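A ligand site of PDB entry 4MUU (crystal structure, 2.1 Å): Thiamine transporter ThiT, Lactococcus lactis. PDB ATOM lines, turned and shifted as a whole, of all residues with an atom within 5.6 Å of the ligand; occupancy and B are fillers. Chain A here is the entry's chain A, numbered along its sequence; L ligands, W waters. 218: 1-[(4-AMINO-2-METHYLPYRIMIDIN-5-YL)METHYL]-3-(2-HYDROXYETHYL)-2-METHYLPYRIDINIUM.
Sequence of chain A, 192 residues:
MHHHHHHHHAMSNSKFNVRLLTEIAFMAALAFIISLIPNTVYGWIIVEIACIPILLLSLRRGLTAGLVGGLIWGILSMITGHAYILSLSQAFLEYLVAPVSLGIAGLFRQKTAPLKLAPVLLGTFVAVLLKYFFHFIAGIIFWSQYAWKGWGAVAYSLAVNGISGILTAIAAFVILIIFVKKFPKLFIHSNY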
ATOM      1  N   ASN A  39      21.792  -3.946 -10.233  1.00  0.00           N
ATOM      2  CA  ASN A  39      22.309  -4.192  -8.880  1.00  0.00           C
ATOM      3  C   ASN A  39      22.904  -5.568  -8.669  1.00  0.00           C
ATOM      4  O   ASN A  39      23.052  -6.011  -7.532  1.00  0.00           O
ATOM      5  CB  ASN A  39      21.188  -3.970  -7.864  1.00  0.00           C
ATOM      6  CG  ASN A  39      20.057  -4.945  -8.020  1.00  0.00           C
ATOM      7  OD1 ASN A  39      20.012  -5.700  -8.982  1.00  0.00           O
ATOM      8  ND2 ASN A  39      19.108  -4.885  -7.120  1.00  0.00           N
ATOM      9  N   TRP A  44      22.292 -14.268  -8.834  1.00  0.00           N
ATOM     10  CA  TRP A  44      21.271 -13.680  -7.980  1.00  0.00           C
ATOM     11  C   TRP A  44      21.825 -13.016  -6.721  1.00  0.00           C
ATOM     12  O   TRP A  44      21.071 -12.633  -5.835  1.00  0.00           O
ATOM     13  CB  TRP A  44      20.210 -14.722  -7.664  1.00  0.00           C
ATOM     14  CG  TRP A  44      19.019 -14.537  -8.570  1.00  0.00           C
ATOM     15  CD1 TRP A  44      18.662 -15.310  -9.621  1.00  0.00           C
ATOM     16  CD2 TRP A  44      18.065 -13.469  -8.497  1.00  0.00           C
ATOM     17  NE1 TRP A  44      17.523 -14.805 -10.223  1.00  0.00           N
ATOM     18  CE2 TRP A  44      17.134 -13.683  -9.552  1.00  0.00           C
ATOM     19  CE3 TRP A  44      17.895 -12.375  -7.650  1.00  0.00           C
ATOM     20  CZ2 TRP A  44      16.040 -12.831  -9.765  1.00  0.00           C
ATOM     21  CZ3 TRP A  44      16.802 -11.523  -7.863  1.00  0.00           C
ATOM     22  CH2 TRP A  44      15.899 -11.761  -8.913  1.00  0.00           C
ATOM     23  N   ILE A  46      22.843  -9.866  -5.221  1.00  0.00           N
ATOM     24  CA  ILE A  46      22.537  -8.487  -5.570  1.00  0.00           C
ATOM     25  C   ILE A  46      22.724  -7.576  -4.364  1.00  0.00           C
ATOM     26  O   ILE A  46      22.799  -8.032  -3.237  1.00  0.00           O
ATOM     27  CB  ILE A  46      21.087  -8.388  -6.038  1.00  0.00           C
ATOM     28  CG1 ILE A  46      20.096  -8.806  -4.942  1.00  0.00           C
ATOM     29  CG2 ILE A  46      20.860  -9.348  -7.242  1.00  0.00           C
ATOM     30  CD1 ILE A  46      18.612  -8.744  -5.397  1.00  0.00           C
ATOM     31  N   GLU A  48      20.439  -4.794  -2.901  1.00  0.00           N
ATOM     32  CA  GLU A  48      19.102  -4.308  -3.170  1.00  0.00           C
ATOM     33  C   GLU A  48      18.864  -2.938  -2.535  1.00  0.00           C
ATOM     34  O   GLU A  48      18.146  -2.786  -1.547  1.00  0.00           O
ATOM     35  CB  GLU A  48      18.046  -5.336  -2.754  1.00  0.00           C
ATOM     36  CG  GLU A  48      16.718  -4.994  -3.457  1.00  0.00           C
ATOM     37  CD  GLU A  48      15.647  -5.999  -3.233  1.00  0.00           C
ATOM     38  OE1 GLU A  48      15.651  -6.638  -2.149  1.00  0.00           O
ATOM     39  OE2 GLU A  48      14.764  -6.121  -4.115  1.00  0.00           O
ATOM     40  N   TYR A  84      10.645 -11.183 -11.274  1.00  0.00           N
ATOM     41  CA  TYR A  84      10.965 -12.494 -11.841  1.00  0.00           C
ATOM     42  C   TYR A  84      10.071 -13.504 -11.142  1.00  0.00           C
ATOM     43  O   TYR A  84      10.241 -13.810  -9.965  1.00  0.00           O
ATOM     44  CB  TYR A  84      12.467 -12.831 -11.647  1.00  0.00           C
ATOM     45  CG  TYR A  84      13.365 -11.832 -12.338  1.00  0.00           C
ATOM     46  CD1 TYR A  84      13.776 -10.669 -11.699  1.00  0.00           C
ATOM     47  CD2 TYR A  84      13.808 -12.038 -13.644  1.00  0.00           C
ATOM     48  CE1 TYR A  84      14.604  -9.737 -12.341  1.00  0.00           C
ATOM     49  CE2 TYR A  84      14.619 -11.121 -14.287  1.00  0.00           C
ATOM     50  CZ  TYR A  84      15.025  -9.973 -13.630  1.00  0.00           C
ATOM     51  OH  TYR A  84      15.836  -9.056 -14.273  1.00  0.00           O
ATOM     52  N   GLN A  90       5.426 -18.437  -5.413  1.00  0.00           N
ATOM     53  CA  GLN A  90       6.745 -17.817  -5.331  1.00  0.00           C
ATOM     54  C   GLN A  90       6.639 -16.291  -5.447  1.00  0.00           C
ATOM     55  O   GLN A  90       7.327 -15.572  -4.712  1.00  0.00           O
ATOM     56  CB  GLN A  90       7.678 -18.427  -6.382  1.00  0.00           C
ATOM     57  CG  GLN A  90       8.990 -17.691  -6.566  1.00  0.00           C
ATOM     58  CD  GLN A  90       8.897 -16.561  -7.568  1.00  0.00           C
ATOM     59  OE1 GLN A  90       7.924 -16.471  -8.340  1.00  0.00           O
ATOM     60  NE2 GLN A  90       9.886 -15.680  -7.549  1.00  0.00           N
ATOM     61  N   GLU A  94       7.883 -13.619  -2.756  1.00  0.00           N
ATOM     62  CA  GLU A  94       9.073 -12.820  -3.011  1.00  0.00           C
ATOM     63  C   GLU A  94       8.784 -11.396  -3.415  1.00  0.00           C
ATOM     64  O   GLU A  94       9.677 -10.565  -3.374  1.00  0.00           O
ATOM     65  CB  GLU A  94       9.949 -13.479  -4.056  1.00  0.00           C
ATOM     66  CG  GLU A  94      10.530 -14.794  -3.603  1.00  0.00           C
ATOM     67  CD  GLU A  94      11.815 -15.060  -4.311  1.00  0.00           C
ATOM     68  OE1 GLU A  94      12.824 -14.522  -3.824  1.00  0.00           O
ATOM     69  OE2 GLU A  94      11.811 -15.759  -5.372  1.00  0.00           O
ATOM     70  N   TYR A  95       7.539 -11.141  -3.822  1.00  0.00           N
ATOM     71  CA  TYR A  95       7.155  -9.834  -4.281  1.00  0.00           C
ATOM     72  C   TYR A  95       5.947  -9.245  -3.554  1.00  0.00           C
ATOM     73  O   TYR A  95       5.535  -8.137  -3.865  1.00  0.00           O
ATOM     74  CB  TYR A  95       6.926  -9.886  -5.784  1.00  0.00           C
ATOM     75  CG  TYR A  95       8.236  -9.958  -6.535  1.00  0.00           C
ATOM     76  CD1 TYR A  95       8.967  -8.818  -6.756  1.00  0.00           C
ATOM     77  CD2 TYR A  95       8.707 -11.167  -7.043  1.00  0.00           C
ATOM     78  CE1 TYR A  95      10.143  -8.855  -7.454  1.00  0.00           C
ATOM     79  CE2 TYR A  95       9.923 -11.222  -7.732  1.00  0.00           C
ATOM     80  CZ  TYR A  95      10.616 -10.049  -7.942  1.00  0.00           C
ATOM     81  OH  TYR A  95      11.793 -10.020  -8.651  1.00  0.00           O
ATOM     82  N   LYS A 131      13.608  -9.844   5.266  1.00  0.00           N
ATOM     83  CA  LYS A 131      13.300  -9.882   3.838  1.00  0.00           C
ATOM     84  C   LYS A 131      14.138 -10.989   3.195  1.00  0.00           C
ATOM     85  O   LYS A 131      13.606 -11.789   2.445  1.00  0.00           O
ATOM     86  CB  LYS A 131      13.600  -8.551   3.155  1.00  0.00           C
ATOM     87  CG  LYS A 131      13.089  -8.468   1.717  1.00  0.00           C
ATOM     88  CD  LYS A 131      13.393  -7.086   1.098  1.00  0.00           C
ATOM     89  CE  LYS A 131      12.713  -6.865  -0.222  1.00  0.00           C
ATOM     90  NZ  LYS A 131      12.908  -7.846  -1.327  1.00  0.00           N
ATOM     91  N   TYR A 132      15.431 -11.039   3.515  1.00  0.00           N
ATOM     92  CA  TYR A 132      16.282 -12.034   2.881  1.00  0.00           C
ATOM     93  C   TYR A 132      16.100 -13.432   3.452  1.00  0.00           C
ATOM     94  O   TYR A 132      16.427 -14.448   2.800  1.00  0.00           O
ATOM     95  CB  TYR A 132      17.733 -11.528   2.783  1.00  0.00           C
ATOM     96  CG  TYR A 132      17.779 -10.693   1.539  1.00  0.00           C
ATOM     97  CD1 TYR A 132      17.308  -9.382   1.532  1.00  0.00           C
ATOM     98  CD2 TYR A 132      18.104 -11.278   0.313  1.00  0.00           C
ATOM     99  CE1 TYR A 132      17.250  -8.651   0.350  1.00  0.00           C
ATOM    100  CE2 TYR A 132      18.061 -10.571  -0.846  1.00  0.00           C
ATOM    101  CZ  TYR A 132      17.629  -9.264  -0.840  1.00  0.00           C
ATOM    102  OH  TYR A 132      17.594  -8.594  -2.039  1.00  0.00           O
ATOM    103  N   PHE A 134      13.011 -14.579   3.822  1.00  0.00           N
ATOM    104  CA  PHE A 134      11.966 -15.069   2.895  1.00  0.00           C
ATOM    105  C   PHE A 134      12.560 -15.420   1.541  1.00  0.00           C
ATOM    106  O   PHE A 134      12.192 -16.446   0.981  1.00  0.00           O
ATOM    107  CB  PHE A 134      10.802 -14.082   2.757  1.00  0.00           C
ATOM    108  CG  PHE A 134       9.965 -13.922   4.019  1.00  0.00           C
ATOM    109  CD1 PHE A 134       9.284 -15.003   4.549  1.00  0.00           C
ATOM    110  CD2 PHE A 134       9.873 -12.704   4.660  1.00  0.00           C
ATOM    111  CE1 PHE A 134       8.522 -14.868   5.689  1.00  0.00           C
ATOM    112  CE2 PHE A 134       9.102 -12.573   5.809  1.00  0.00           C
ATOM    113  CZ  PHE A 134       8.422 -13.660   6.318  1.00  0.00           C
ATOM    114  N   HIS A 135      13.499 -14.633   1.037  1.00  0.00           N
ATOM    115  CA  HIS A 135      14.159 -15.036  -0.220  1.00  0.00           C
ATOM    116  C   HIS A 135      14.911 -16.325  -0.081  1.00  0.00           C
ATOM    117  O   HIS A 135      14.913 -17.139  -1.008  1.00  0.00           O
ATOM    118  CB  HIS A 135      15.114 -13.967  -0.759  1.00  0.00           C
ATOM    119  CG  HIS A 135      14.417 -12.689  -1.092  1.00  0.00           C
ATOM    120  ND1 HIS A 135      13.369 -12.632  -1.996  1.00  0.00           N
ATOM    121  CD2 HIS A 135      14.611 -11.426  -0.655  1.00  0.00           C
ATOM    122  CE1 HIS A 135      12.943 -11.384  -2.069  1.00  0.00           C
ATOM    123  NE2 HIS A 135      13.680 -10.636  -1.268  1.00  0.00           N
ATOM    124  N   PHE A 136      15.567 -16.500   1.068  1.00  0.00           N
ATOM    125  CA  PHE A 136      16.271 -17.743   1.372  1.00  0.00           C
ATOM    126  C   PHE A 136      15.337 -18.956   1.291  1.00  0.00           C
ATOM    127  O   PHE A 136      15.666 -19.977   0.668  1.00  0.00           O
ATOM    128  CB  PHE A 136      16.934 -17.650   2.763  1.00  0.00           C
ATOM    129  CG  PHE A 136      17.355 -18.992   3.330  1.00  0.00           C
ATOM    130  CD1 PHE A 136      18.349 -19.734   2.705  1.00  0.00           C
ATOM    131  CD2 PHE A 136      16.760 -19.486   4.488  1.00  0.00           C
ATOM    132  CE1 PHE A 136      18.742 -20.963   3.215  1.00  0.00           C
ATOM    133  CE2 PHE A 136      17.164 -20.727   5.013  1.00  0.00           C
ATOM    134  CZ  PHE A 136      18.146 -21.444   4.379  1.00  0.00           C
ATOM    135  N   ALA A 138      12.540 -19.045  -0.304  1.00  0.00           N
ATOM    136  CA  ALA A 138      12.131 -19.096  -1.708  1.00  0.00           C
ATOM    137  C   ALA A 138      13.196 -19.739  -2.556  1.00  0.00           C
ATOM    138  O   ALA A 138      12.917 -20.353  -3.598  1.00  0.00           O
ATOM    139  CB  ALA A 138      11.886 -17.672  -2.202  1.00  0.00           C
ATOM    140  N   GLY A 139      14.445 -19.585  -2.120  1.00  0.00           N
ATOM    141  CA  GLY A 139      15.561 -20.100  -2.867  1.00  0.00           C
ATOM    142  C   GLY A 139      15.566 -21.614  -2.767  1.00  0.00           C
ATOM    143  O   GLY A 139      15.765 -22.301  -3.751  1.00  0.00           O
ATOM    144  N   TRP A 143      14.263 -22.091  -6.579  1.00  0.00           N
ATOM    145  CA  TRP A 143      15.426 -21.755  -7.407  1.00  0.00           C
ATOM    146  C   TRP A 143      16.528 -22.784  -7.321  1.00  0.00           C
ATOM    147  O   TRP A 143      17.638 -22.517  -7.737  1.00  0.00           O
ATOM    148  CB  TRP A 143      16.004 -20.380  -6.956  1.00  0.00           C
ATOM    149  CG  TRP A 143      15.056 -19.254  -7.120  1.00  0.00           C
ATOM    150  CD1 TRP A 143      14.120 -18.808  -6.212  1.00  0.00           C
ATOM    151  CD2 TRP A 143      14.924 -18.398  -8.276  1.00  0.00           C
ATOM    152  NE1 TRP A 143      13.409 -17.762  -6.747  1.00  0.00           N
ATOM    153  CE2 TRP A 143      13.883 -17.485  -7.997  1.00  0.00           C
ATOM    154  CE3 TRP A 143      15.584 -18.337  -9.512  1.00  0.00           C
ATOM    155  CZ2 TRP A 143      13.511 -16.497  -8.892  1.00  0.00           C
ATOM    156  CZ3 TRP A 143      15.192 -17.353 -10.416  1.00  0.00           C
ATOM    157  CH2 TRP A 143      14.168 -16.449 -10.096  1.00  0.00           C
ATOM    158  N   TYR A 156      23.158 -23.496  -1.405  1.00  0.00           N
ATOM    159  CA  TYR A 156      23.075 -22.486  -2.450  1.00  0.00           C
ATOM    160  C   TYR A 156      22.236 -21.270  -2.000  1.00  0.00           C
ATOM    161  O   TYR A 156      22.662 -20.118  -2.140  1.00  0.00           O
ATOM    162  CB  TYR A 156      22.469 -23.111  -3.710  1.00  0.00           C
ATOM    163  CG  TYR A 156      22.279 -22.155  -4.854  1.00  0.00           C
ATOM    164  CD1 TYR A 156      23.371 -21.526  -5.449  1.00  0.00           C
ATOM    165  CD2 TYR A 156      21.021 -21.898  -5.361  1.00  0.00           C
ATOM    166  CE1 TYR A 156      23.204 -20.665  -6.523  1.00  0.00           C
ATOM    167  CE2 TYR A 156      20.837 -21.040  -6.432  1.00  0.00           C
ATOM    168  CZ  TYR A 156      21.912 -20.419  -7.006  1.00  0.00           C
ATOM    169  OH  TYR A 156      21.707 -19.545  -8.060  1.00  0.00           O
ATOM    170  N   SER A 157      21.044 -21.537  -1.478  1.00  0.00           N
ATOM    171  CA  SER A 157      20.157 -20.434  -1.110  1.00  0.00           C
ATOM    172  C   SER A 157      20.768 -19.597   0.006  1.00  0.00           C
ATOM    173  O   SER A 157      20.709 -18.377  -0.050  1.00  0.00           O
ATOM    174  CB  SER A 157      18.795 -20.918  -0.683  1.00  0.00           C
ATOM    175  OG  SER A 157      17.931 -19.808  -0.710  1.00  0.00           O
ATOM    176  N   VAL A 160      23.605 -17.488  -1.560  1.00  0.00           N
ATOM    177  CA  VAL A 160      23.081 -16.469  -2.448  1.00  0.00           C
ATOM    178  C   VAL A 160      22.360 -15.398  -1.636  1.00  0.00           C
ATOM    179  O   VAL A 160      22.675 -14.232  -1.760  1.00  0.00           O
ATOM    180  CB  VAL A 160      22.152 -17.056  -3.562  1.00  0.00           C
ATOM    181  CG1 VAL A 160      21.448 -15.988  -4.300  1.00  0.00           C
ATOM    182  CG2 VAL A 160      23.004 -17.916  -4.584  1.00  0.00           C
ATOM    183  N   ASN A 161      21.403 -15.803  -0.814  1.00  0.00           N
ATOM    184  CA  ASN A 161      20.521 -14.832  -0.199  1.00  0.00           C
ATOM    185  C   ASN A 161      21.164 -14.226   1.057  1.00  0.00           C
ATOM    186  O   ASN A 161      20.967 -13.057   1.362  1.00  0.00           O
ATOM    187  CB  ASN A 161      19.149 -15.493   0.024  1.00  0.00           C
ATOM    188  CG  ASN A 161      18.470 -15.787  -1.288  1.00  0.00           C
ATOM    189  OD1 ASN A 161      18.209 -16.944  -1.632  1.00  0.00           O
ATOM    190  ND2 ASN A 161      18.253 -14.751  -2.064  1.00  0.00           N
HETATM  191  CM2 218 L   1      18.855 -18.860  -4.897  1.00  0.00           C
HETATM  192  C2A 218 L   1      17.850 -17.753  -5.280  1.00  0.00           C
HETATM  193  N1A 218 L   1      17.901 -17.202  -6.501  1.00  0.00           N
HETATM  194  C6A 218 L   1      17.027 -16.213  -6.829  1.00  0.00           C
HETATM  195  C5A 218 L   1      16.060 -15.815  -5.899  1.00  0.00           C
HETATM  196  C7A 218 L   1      15.057 -14.715  -6.303  1.00  0.00           C
HETATM  197  N3  218 L   1      15.245 -13.476  -5.582  1.00  0.00           N
HETATM  198  C2  218 L   1      16.307 -13.359  -4.731  1.00  0.00           C
HETATM  199  C1  218 L   1      16.510 -12.157  -3.993  1.00  0.00           C
HETATM  200  C6  218 L   1      15.588 -11.081  -4.126  1.00  0.00           C
HETATM  201  C5  218 L   1      14.501 -11.279  -5.024  1.00  0.00           C
HETATM  202  CM6 218 L   1      13.449 -10.156  -5.224  1.00  0.00           C
HETATM  203  CM7 218 L   1      13.926  -9.134  -6.300  1.00  0.00           C
HETATM  204  OM7 218 L   1      15.139  -8.476  -5.848  1.00  0.00           O
HETATM  205  C4  218 L   1      14.357 -12.514  -5.734  1.00  0.00           C
HETATM  206  CM4 218 L   1      13.162 -12.739  -6.721  1.00  0.00           C
HETATM  207  C4A 218 L   1      16.062 -16.461  -4.630  1.00  0.00           C
HETATM  208  N4A 218 L   1      15.135 -16.128  -3.573  1.00  0.00           N
HETATM  209  N3A 218 L   1      16.966 -17.423  -4.364  1.00  0.00           N
HETATM  210  O   HOH W   1      19.254 -18.806  -8.552  1.00  0.00           O
HETATM  211  O   HOH W   2      19.611 -12.854  -3.470  1.00  0.00           O
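The backbone carbonyl oxygen of His 135 lies within hydrogen-bond range of a nitrogen (N4A) of the ligand (2.8 Å). A nitrogen (N4A) of the ligand lies within hydrogen-bond range of the side-chain carboxylate (OE1) of Glu 94. The side-chain amide oxygen (OD1) of Asn 161 sits close to a nitrogen (N3A) of the ligand, 3.0 Å away. OE2 of Glu 48 sits at hydrogen-bond distance from OM7 of the ligand, 2.9 Å away.
The side-chain amide nitrogen (NE2) of Gln 90 is in hydrogen-bond range of the side-chain carboxylate (OE2) of Glu 94. ND1 of His 135 lies within hydrogen-bond range of OE1 of Glu 94 (2.7 Å). The side-chain carboxylate (OE1) of Glu 48 is in salt-bridge range of the side-chain amino group (NZ) of Lys 131 (3.1 Å). The backbone NH of Tyr 84 lies within hydrogen-bond range of the side-chain hydroxyl of Tyr 95. The side-chain amide oxygen (OD1) of Asn 161 lies close to the backbone carbonyl oxygen (O) of His 135 (3.4 Å). The side-chain carboxylate (OE2) of Glu 94 lies within hydrogen-bond range of the indole nitrogen (NE1) of Trp 143, at 2.9 Å. The side-chain carboxylate of Glu 48 is in hydrogen-bond range of the side-chain hydroxyl of Tyr 132 (2.8 Å). A ring nitrogen (NE2) of His 135 sits at hydrogen-bond distance from the side-chain amino group (NZ) of Lys 131.
Merely in contact with the ligand: Trp 44 (3.1 Å), Ile 46 (3.5 Å), Tyr 95 (3.3 Å), Tyr 132 (3.8 Å), Ala 138 (3.8 Å), Gly 139 (3.4 Å), Trp 143 (3.4 Å), Tyr 156 (3.3 Å) and Val 160 (3.9 Å). Hydrophobic or aromatic side chains within 4 Å of the ligand: Trp 44, Ile 46, Tyr 95, Tyr 132, His 135, Ala 138, Trp 143, Tyr 156 and Val 160. Of the 20 residues printed, 13 come within 4 Å of the ligand.
Water W1 bridges OH of Tyr 156 (2.6 Å) and N1A of the ligand (2.9 Å). Water W2 lies within hydrogen-bond range of the side-chain amide nitrogen of Asn 161 (2.7 Å) and the backbone carbonyl oxygen of Trp 44 (2.8 Å).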
